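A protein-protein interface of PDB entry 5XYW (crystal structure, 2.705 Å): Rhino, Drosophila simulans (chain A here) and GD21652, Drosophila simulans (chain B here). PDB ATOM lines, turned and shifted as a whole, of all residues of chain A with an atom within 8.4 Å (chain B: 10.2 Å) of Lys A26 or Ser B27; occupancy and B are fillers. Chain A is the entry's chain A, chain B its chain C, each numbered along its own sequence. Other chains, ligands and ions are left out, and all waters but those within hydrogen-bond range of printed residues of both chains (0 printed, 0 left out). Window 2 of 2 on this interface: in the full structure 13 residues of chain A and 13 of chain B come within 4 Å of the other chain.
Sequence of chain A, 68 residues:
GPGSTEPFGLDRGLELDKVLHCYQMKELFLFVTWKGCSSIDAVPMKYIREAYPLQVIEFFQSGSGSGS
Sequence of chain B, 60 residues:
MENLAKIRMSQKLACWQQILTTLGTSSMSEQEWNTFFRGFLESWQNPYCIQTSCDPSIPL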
ATOM      1  N   TYR A  23       5.999   2.198  13.559  1.00  0.00           N
ATOM      2  CA  TYR A  23       5.014   1.816  12.538  1.00  0.00           C
ATOM      3  C   TYR A  23       4.702   2.989  11.604  1.00  0.00           C
ATOM      4  O   TYR A  23       4.330   4.087  12.017  1.00  0.00           O
ATOM      5  CB  TYR A  23       3.722   1.273  13.180  1.00  0.00           C
ATOM      6  CG  TYR A  23       2.769   0.696  12.161  1.00  0.00           C
ATOM      7  CD1 TYR A  23       3.072  -0.486  11.492  1.00  0.00           C
ATOM      8  CD2 TYR A  23       1.579   1.353  11.829  1.00  0.00           C
ATOM      9  CE1 TYR A  23       2.211  -1.008  10.513  1.00  0.00           C
ATOM     10  CE2 TYR A  23       0.708   0.830  10.875  1.00  0.00           C
ATOM     11  CZ  TYR A  23       1.037  -0.341  10.215  1.00  0.00           C
ATOM     12  OH  TYR A  23       0.171  -0.834   9.271  1.00  0.00           O
ATOM     13  N   GLN A  24       4.887   2.740  10.323  1.00  0.00           N
ATOM     14  CA  GLN A  24       4.760   3.789   9.331  1.00  0.00           C
ATOM     15  C   GLN A  24       3.358   3.850   8.777  1.00  0.00           C
ATOM     16  O   GLN A  24       2.911   2.897   8.152  1.00  0.00           O
ATOM     17  CB  GLN A  24       5.751   3.560   8.182  1.00  0.00           C
ATOM     18  CG  GLN A  24       5.628   4.550   7.058  1.00  0.00           C
ATOM     19  CD  GLN A  24       6.207   5.891   7.427  1.00  0.00           C
ATOM     20  OE1 GLN A  24       7.345   5.979   7.886  1.00  0.00           O
ATOM     21  NE2 GLN A  24       5.418   6.947   7.255  1.00  0.00           N
ATOM     22  N   MET A  25       2.669   4.967   9.009  1.00  0.00           N
ATOM     23  CA  MET A  25       1.397   5.268   8.336  1.00  0.00           C
ATOM     24  C   MET A  25       1.584   6.558   7.526  1.00  0.00           C
ATOM     25  O   MET A  25       2.692   6.833   7.060  1.00  0.00           O
ATOM     26  CB  MET A  25       0.247   5.396   9.347  1.00  0.00           C
ATOM     27  CG  MET A  25       0.111   4.189  10.253  1.00  0.00           C
ATOM     28  SD  MET A  25      -1.326   4.127  11.358  1.00  0.00           S
ATOM     29  CE  MET A  25      -2.643   4.481  10.196  1.00  0.00           C
ATOM     30  N   LYS A  26       0.523   7.345   7.353  1.00  0.00           N
ATOM     31  CA  LYS A  26       0.669   8.702   6.820  1.00  0.00           C
ATOM     32  C   LYS A  26       1.742   9.410   7.633  1.00  0.00           C
ATOM     33  O   LYS A  26       2.541  10.171   7.111  1.00  0.00           O
ATOM     34  CB  LYS A  26      -0.645   9.489   6.878  1.00  0.00           C
ATOM     35  CG  LYS A  26      -1.445   9.267   8.177  1.00  0.00           C
ATOM     36  CD  LYS A  26      -2.711  10.138   8.272  1.00  0.00           C
ATOM     37  CE  LYS A  26      -2.390  11.618   8.516  1.00  0.00           C
ATOM     38  NZ  LYS A  26      -3.626  12.441   8.743  1.00  0.00           N
ATOM     39  N   GLU A  27       1.751   9.151   8.928  1.00  0.00           N
ATOM     40  CA  GLU A  27       2.838   9.595   9.750  1.00  0.00           C
ATOM     41  C   GLU A  27       3.570   8.373  10.282  1.00  0.00           C
ATOM     42  O   GLU A  27       2.986   7.296  10.419  1.00  0.00           O
ATOM     43  CB  GLU A  27       2.338  10.495  10.873  1.00  0.00           C
ATOM     44  CG  GLU A  27       2.100  11.900  10.387  1.00  0.00           C
ATOM     45  CD  GLU A  27       1.762  12.847  11.505  1.00  0.00           C
ATOM     46  OE1 GLU A  27       1.903  12.441  12.676  1.00  0.00           O
ATOM     47  OE2 GLU A  27       1.353  13.993  11.212  1.00  0.00           O
ATOM     48  N   LEU A  28       4.865   8.542  10.519  1.00  0.00           N
ATOM     49  CA  LEU A  28       5.656   7.521  11.160  1.00  0.00           C
ATOM     50  C   LEU A  28       5.432   7.619  12.669  1.00  0.00           C
ATOM     51  O   LEU A  28       5.438   8.705  13.248  1.00  0.00           O
ATOM     52  CB  LEU A  28       7.120   7.699  10.791  1.00  0.00           C
ATOM     53  CG  LEU A  28       8.157   6.674  11.218  1.00  0.00           C
ATOM     54  CD1 LEU A  28       7.698   5.242  11.000  1.00  0.00           C
ATOM     55  CD2 LEU A  28       9.409   6.941  10.439  1.00  0.00           C
ATOM     56  N   PHE A  29       5.191   6.487  13.305  1.00  0.00           N
ATOM     57  CA  PHE A  29       4.980   6.483  14.743  1.00  0.00           C
ATOM     58  C   PHE A  29       6.078   5.721  15.429  1.00  0.00           C
ATOM     59  O   PHE A  29       6.505   4.677  14.950  1.00  0.00           O
ATOM     60  CB  PHE A  29       3.628   5.867  15.105  1.00  0.00           C
ATOM     61  CG  PHE A  29       2.509   6.841  15.066  1.00  0.00           C
ATOM     62  CD1 PHE A  29       2.323   7.729  16.114  1.00  0.00           C
ATOM     63  CD2 PHE A  29       1.667   6.897  13.968  1.00  0.00           C
ATOM     64  CE1 PHE A  29       1.301   8.652  16.070  1.00  0.00           C
ATOM     65  CE2 PHE A  29       0.656   7.817  13.907  1.00  0.00           C
ATOM     66  CZ  PHE A  29       0.453   8.692  14.956  1.00  0.00           C
ATOM     67  N   LYS A  46       8.101  13.048  13.954  1.00  0.00           N
ATOM     68  CA  LYS A  46       8.545  14.430  13.869  1.00  0.00           C
ATOM     69  C   LYS A  46       8.769  15.048  15.246  1.00  0.00           C
ATOM     70  O   LYS A  46       9.812  15.662  15.519  1.00  0.00           O
ATOM     71  CB  LYS A  46       7.520  15.228  13.070  1.00  0.00           C
ATOM     72  CG  LYS A  46       6.988  14.441  11.861  1.00  0.00           C
ATOM     73  CD  LYS A  46       5.976  15.225  11.028  1.00  0.00           C
ATOM     74  CE  LYS A  46       5.660  14.496   9.717  1.00  0.00           C
ATOM     75  NZ  LYS A  46       4.518  15.101   8.957  1.00  0.00           N
ATOM     76  N   TRP B  16      -2.726   2.093  19.741  1.00  0.00           N
ATOM     77  CA  TRP B  16      -3.616   2.290  18.626  1.00  0.00           C
ATOM     78  C   TRP B  16      -4.597   3.419  18.917  1.00  0.00           C
ATOM     79  O   TRP B  16      -4.943   4.196  18.026  1.00  0.00           O
ATOM     80  CB  TRP B  16      -4.362   1.018  18.300  1.00  0.00           C
ATOM     81  CG  TRP B  16      -5.223   1.178  17.110  1.00  0.00           C
ATOM     82  CD1 TRP B  16      -6.581   1.236  17.074  1.00  0.00           C
ATOM     83  CD2 TRP B  16      -4.781   1.290  15.754  1.00  0.00           C
ATOM     84  NE1 TRP B  16      -7.017   1.363  15.772  1.00  0.00           N
ATOM     85  CE2 TRP B  16      -5.928   1.404  14.946  1.00  0.00           C
ATOM     86  CE3 TRP B  16      -3.521   1.289  15.149  1.00  0.00           C
ATOM     87  CZ2 TRP B  16      -5.856   1.529  13.567  1.00  0.00           C
ATOM     88  CZ3 TRP B  16      -3.451   1.412  13.778  1.00  0.00           C
ATOM     89  CH2 TRP B  16      -4.609   1.534  12.999  1.00  0.00           C
ATOM     90  N   ILE B  19      -2.917   6.531  18.419  1.00  0.00           N
ATOM     91  CA  ILE B  19      -2.764   6.755  16.993  1.00  0.00           C
ATOM     92  C   ILE B  19      -4.045   7.396  16.427  1.00  0.00           C
ATOM     93  O   ILE B  19      -3.991   8.416  15.719  1.00  0.00           O
ATOM     94  CB  ILE B  19      -2.399   5.418  16.267  1.00  0.00           C
ATOM     95  CG1 ILE B  19      -0.912   5.094  16.502  1.00  0.00           C
ATOM     96  CG2 ILE B  19      -2.617   5.498  14.763  1.00  0.00           C
ATOM     97  CD1 ILE B  19      -0.429   3.752  15.881  1.00  0.00           C
ATOM     98  N   LEU B  20      -5.196   6.822  16.777  1.00  0.00           N
ATOM     99  CA  LEU B  20      -6.485   7.325  16.312  1.00  0.00           C
ATOM    100  C   LEU B  20      -6.670   8.763  16.772  1.00  0.00           C
ATOM    101  O   LEU B  20      -7.069   9.638  16.000  1.00  0.00           O
ATOM    102  CB  LEU B  20      -7.616   6.455  16.848  1.00  0.00           C
ATOM    103  CG  LEU B  20      -7.653   4.980  16.430  1.00  0.00           C
ATOM    104  CD1 LEU B  20      -8.787   4.236  17.126  1.00  0.00           C
ATOM    105  CD2 LEU B  20      -7.763   4.863  14.923  1.00  0.00           C
ATOM    106  N   THR B  21      -6.275   9.027  18.009  1.00  0.00           N
ATOM    107  CA  THR B  21      -6.369  10.381  18.544  1.00  0.00           C
ATOM    108  C   THR B  21      -5.461  11.366  17.807  1.00  0.00           C
ATOM    109  O   THR B  21      -5.835  12.520  17.624  1.00  0.00           O
ATOM    110  CB  THR B  21      -6.034  10.417  20.051  1.00  0.00           C
ATOM    111  OG1 THR B  21      -6.918   9.541  20.753  1.00  0.00           O
ATOM    112  CG2 THR B  21      -6.189  11.817  20.607  1.00  0.00           C
ATOM    113  N   THR B  22      -4.292  10.909  17.358  1.00  0.00           N
ATOM    114  CA  THR B  22      -3.329  11.816  16.732  1.00  0.00           C
ATOM    115  C   THR B  22      -3.748  12.139  15.315  1.00  0.00           C
ATOM    116  O   THR B  22      -3.707  13.296  14.895  1.00  0.00           O
ATOM    117  CB  THR B  22      -1.887  11.215  16.699  1.00  0.00           C
ATOM    118  OG1 THR B  22      -1.551  10.682  17.983  1.00  0.00           O
ATOM    119  CG2 THR B  22      -0.853  12.269  16.305  1.00  0.00           C
ATOM    120  N   LEU B  23      -4.188  11.115  14.590  1.00  0.00           N
ATOM    121  CA  LEU B  23      -4.627  11.325  13.211  1.00  0.00           C
ATOM    122  C   LEU B  23      -6.073  11.805  13.109  1.00  0.00           C
ATOM    123  O   LEU B  23      -6.386  12.621  12.241  1.00  0.00           O
ATOM    124  CB  LEU B  23      -4.467  10.046  12.388  1.00  0.00           C
ATOM    125  CG  LEU B  23      -3.135   9.324  12.514  1.00  0.00           C
ATOM    126  CD1 LEU B  23      -3.148   8.073  11.682  1.00  0.00           C
ATOM    127  CD2 LEU B  23      -1.972  10.253  12.129  1.00  0.00           C
ATOM    128  N   GLY B  24      -6.939  11.319  13.999  1.00  0.00           N
ATOM    129  CA  GLY B  24      -8.370  11.557  13.868  1.00  0.00           C
ATOM    130  C   GLY B  24      -9.076  10.525  13.008  1.00  0.00           C
ATOM    131  O   GLY B  24      -8.657  10.241  11.901  1.00  0.00           O
ATOM    132  N   THR B  25     -10.146   9.957  13.540  1.00  0.00           N
ATOM    133  CA  THR B  25     -10.937   8.929  12.861  1.00  0.00           C
ATOM    134  C   THR B  25     -11.396   9.358  11.496  1.00  0.00           C
ATOM    135  O   THR B  25     -11.357   8.590  10.538  1.00  0.00           O
ATOM    136  CB  THR B  25     -12.160   8.587  13.677  1.00  0.00           C
ATOM    137  OG1 THR B  25     -12.838   9.802  14.007  1.00  0.00           O
ATOM    138  CG2 THR B  25     -11.737   7.909  14.965  1.00  0.00           C
ATOM    139  N   SER B  26     -11.815  10.613  11.408  1.00  0.00           N
ATOM    140  CA  SER B  26     -12.321  11.176  10.164  1.00  0.00           C
ATOM    141  C   SER B  26     -11.245  11.271   9.089  1.00  0.00           C
ATOM    142  O   SER B  26     -11.483  11.792   8.008  1.00  0.00           O
ATOM    143  CB  SER B  26     -12.900  12.561  10.415  1.00  0.00           C
ATOM    144  OG  SER B  26     -11.849  13.461  10.719  1.00  0.00           O
ATOM    145  N   SER B  27     -10.059  10.770   9.388  1.00  0.00           N
ATOM    146  CA  SER B  27      -8.923  10.925   8.500  1.00  0.00           C
ATOM    147  C   SER B  27      -8.924   9.894   7.389  1.00  0.00           C
ATOM    148  O   SER B  27      -8.352  10.124   6.323  1.00  0.00           O
ATOM    149  CB  SER B  27      -7.619  10.832   9.300  1.00  0.00           C
ATOM    150  OG  SER B  27      -6.509  10.590   8.461  1.00  0.00           O
ATOM    151  N   MET B  28      -9.567   8.759   7.644  1.00  0.00           N
ATOM    152  CA  MET B  28      -9.591   7.663   6.685  1.00  0.00           C
ATOM    153  C   MET B  28     -10.974   7.055   6.673  1.00  0.00           C
ATOM    154  O   MET B  28     -11.790   7.300   7.562  1.00  0.00           O
ATOM    155  CB  MET B  28      -8.608   6.531   7.028  1.00  0.00           C
ATOM    156  CG  MET B  28      -7.190   6.922   7.386  1.00  0.00           C
ATOM    157  SD  MET B  28      -6.200   5.439   7.552  1.00  0.00           S
ATOM    158  CE  MET B  28      -5.733   5.357   5.842  1.00  0.00           C
ATOM    159  N   SER B  29     -11.246   6.270   5.646  1.00  0.00           N
ATOM    160  CA  SER B  29     -12.407   5.399   5.684  1.00  0.00           C
ATOM    161  C   SER B  29     -12.108   4.238   6.626  1.00  0.00           C
ATOM    162  O   SER B  29     -10.970   4.016   7.012  1.00  0.00           O
ATOM    163  CB  SER B  29     -12.755   4.892   4.287  1.00  0.00           C
ATOM    164  OG  SER B  29     -11.881   3.856   3.888  1.00  0.00           O
ATOM    165  N   GLU B  30     -13.140   3.503   7.012  1.00  0.00           N
ATOM    166  CA  GLU B  30     -12.981   2.359   7.897  1.00  0.00           C
ATOM    167  C   GLU B  30     -12.211   1.226   7.213  1.00  0.00           C
ATOM    168  O   GLU B  30     -11.525   0.457   7.875  1.00  0.00           O
ATOM    169  CB  GLU B  30     -14.339   1.869   8.425  1.00  0.00           C
ATOM    170  CG  GLU B  30     -15.451   1.646   7.400  1.00  0.00           C
ATOM    171  CD  GLU B  30     -16.121   2.939   6.941  1.00  0.00           C
ATOM    172  OE1 GLU B  30     -15.551   4.030   7.168  1.00  0.00           O
ATOM    173  OE2 GLU B  30     -17.238   2.862   6.384  1.00  0.00           O
ATOM    174  N   GLN B  31     -12.316   1.129   5.891  1.00  0.00           N
ATOM    175  CA  GLN B  31     -11.610   0.091   5.143  1.00  0.00           C
ATOM    176  C   GLN B  31     -10.102   0.290   5.315  1.00  0.00           C
ATOM    177  O   GLN B  31      -9.353  -0.628   5.690  1.00  0.00           O
ATOM    178  CB  GLN B  31     -11.975   0.191   3.656  1.00  0.00           C
ATOM    179  CG  GLN B  31     -11.083  -0.615   2.710  1.00  0.00           C
ATOM    180  CD  GLN B  31     -11.253  -0.230   1.227  1.00  0.00           C
ATOM    181  OE1 GLN B  31     -11.236   0.954   0.873  1.00  0.00           O
ATOM    182  NE2 GLN B  31     -11.377  -1.234   0.359  1.00  0.00           N
ATOM    183  N   GLU B  32      -9.710   1.537   5.107  1.00  0.00           N
ATOM    184  CA  GLU B  32      -8.361   2.026   5.253  1.00  0.00           C
ATOM    185  C   GLU B  32      -7.842   1.763   6.659  1.00  0.00           C
ATOM    186  O   GLU B  32      -6.800   1.115   6.847  1.00  0.00           O
ATOM    187  CB  GLU B  32      -8.379   3.508   4.946  1.00  0.00           C
ATOM    188  CG  GLU B  32      -8.330   3.819   3.466  1.00  0.00           C
ATOM    189  CD  GLU B  32      -8.774   5.237   3.166  1.00  0.00           C
ATOM    190  OE1 GLU B  32      -9.944   5.426   2.766  1.00  0.00           O
ATOM    191  OE2 GLU B  32      -7.969   6.167   3.337  1.00  0.00           O
ATOM    192  N   TRP B  33      -8.595   2.254   7.642  1.00  0.00           N
ATOM    193  CA  TRP B  33      -8.252   2.074   9.046  1.00  0.00           C
ATOM    194  C   TRP B  33      -8.011   0.602   9.343  1.00  0.00           C
ATOM    195  O   TRP B  33      -7.095   0.258  10.064  1.00  0.00           O
ATOM    196  CB  TRP B  33      -9.329   2.614   9.968  1.00  0.00           C
ATOM    197  CG  TRP B  33      -9.252   4.082  10.239  1.00  0.00           C
ATOM    198  CD1 TRP B  33     -10.176   5.033   9.903  1.00  0.00           C
ATOM    199  CD2 TRP B  33      -8.193   4.770  10.909  1.00  0.00           C
ATOM    200  NE1 TRP B  33      -9.759   6.275  10.332  1.00  0.00           N
ATOM    201  CE2 TRP B  33      -8.539   6.142  10.941  1.00  0.00           C
ATOM    202  CE3 TRP B  33      -6.974   4.369  11.461  1.00  0.00           C
ATOM    203  CZ2 TRP B  33      -7.713   7.106  11.514  1.00  0.00           C
ATOM    204  CZ3 TRP B  33      -6.157   5.329  12.034  1.00  0.00           C
ATOM    205  CH2 TRP B  33      -6.532   6.682  12.060  1.00  0.00           C
ATOM    206  N   PHE B  36      -4.602  -0.713   7.727  1.00  0.00           N
ATOM    207  CA  PHE B  36      -3.541  -0.246   8.607  1.00  0.00           C
ATOM    208  C   PHE B  36      -3.540  -0.904   9.985  1.00  0.00           C
ATOM    209  O   PHE B  36      -2.485  -1.180  10.509  1.00  0.00           O
ATOM    210  CB  PHE B  36      -3.591   1.272   8.777  1.00  0.00           C
ATOM    211  CG  PHE B  36      -2.958   2.019   7.644  1.00  0.00           C
ATOM    212  CD1 PHE B  36      -1.601   1.855   7.389  1.00  0.00           C
ATOM    213  CD2 PHE B  36      -3.686   2.891   6.848  1.00  0.00           C
ATOM    214  CE1 PHE B  36      -0.991   2.526   6.357  1.00  0.00           C
ATOM    215  CE2 PHE B  36      -3.064   3.572   5.807  1.00  0.00           C
ATOM    216  CZ  PHE B  36      -1.727   3.391   5.558  1.00  0.00           C
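The backbone NH of Phe A29 lies within hydrogen-bond range of the backbone carbonyl oxygen of Tyr A23 (2.9 Å).
Among the printed residues, pairs that only touch across the chains: Met A25 with Ile B19, Met A25 with Leu B23, Met A25 with Phe B36, Lys A26 with Leu B23 and Phe A29 with Thr B22.
O of Phe B36 lies within hydrogen-bond range of OH of Tyr A23 (3.0 Å).
The side-chain amino group (NZ) of Lys A26 is in hydrogen-bond range of the side-chain hydroxyl (OG) of Ser B27 (3.4 Å).
Of the 17 printed residues of chain B, 5 touch a printed residue of chain A.
Hydrophobic or aromatic side chains of chain B that line the printed part of chain A: Ile B19, Leu B23 and Phe B36.
Of the 8 printed residues of chain A, 4 touch a printed residue of chain B.
Hydrophobic or aromatic side chains of chain A within 4 Å of the printed part of chain B: Tyr A23, Met A25 and Phe A29.
Among the printed residues, no Asp or Glu carboxylate lies within 4 Å of a Lys or Arg side-chain nitrogen of the other chain.
Lys A26 touches just these residues of chain B: Leu B23 (3.9 Å) and Ser B27 (3.4 Å).
Ser B27 touches just one residue of chain A: Lys A26 (3.4 Å).
Of chain B, only Ile B19, Leu B23 and Phe B36 come within 4 Å of Met A25.
No residue of chain B comes within 4 Å of Glu A27.
No residue of chain A comes within 4 Å of Ser B26.
Of the printed residues of chain A, Ile B19 touches Met A25.
Of the printed residues of chain B, Tyr A23 touches Phe B36 (3.0 Å).
The nearest printed residue of chain A that does not touch Leu B23 is Phe A29 (4.0002 Å).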
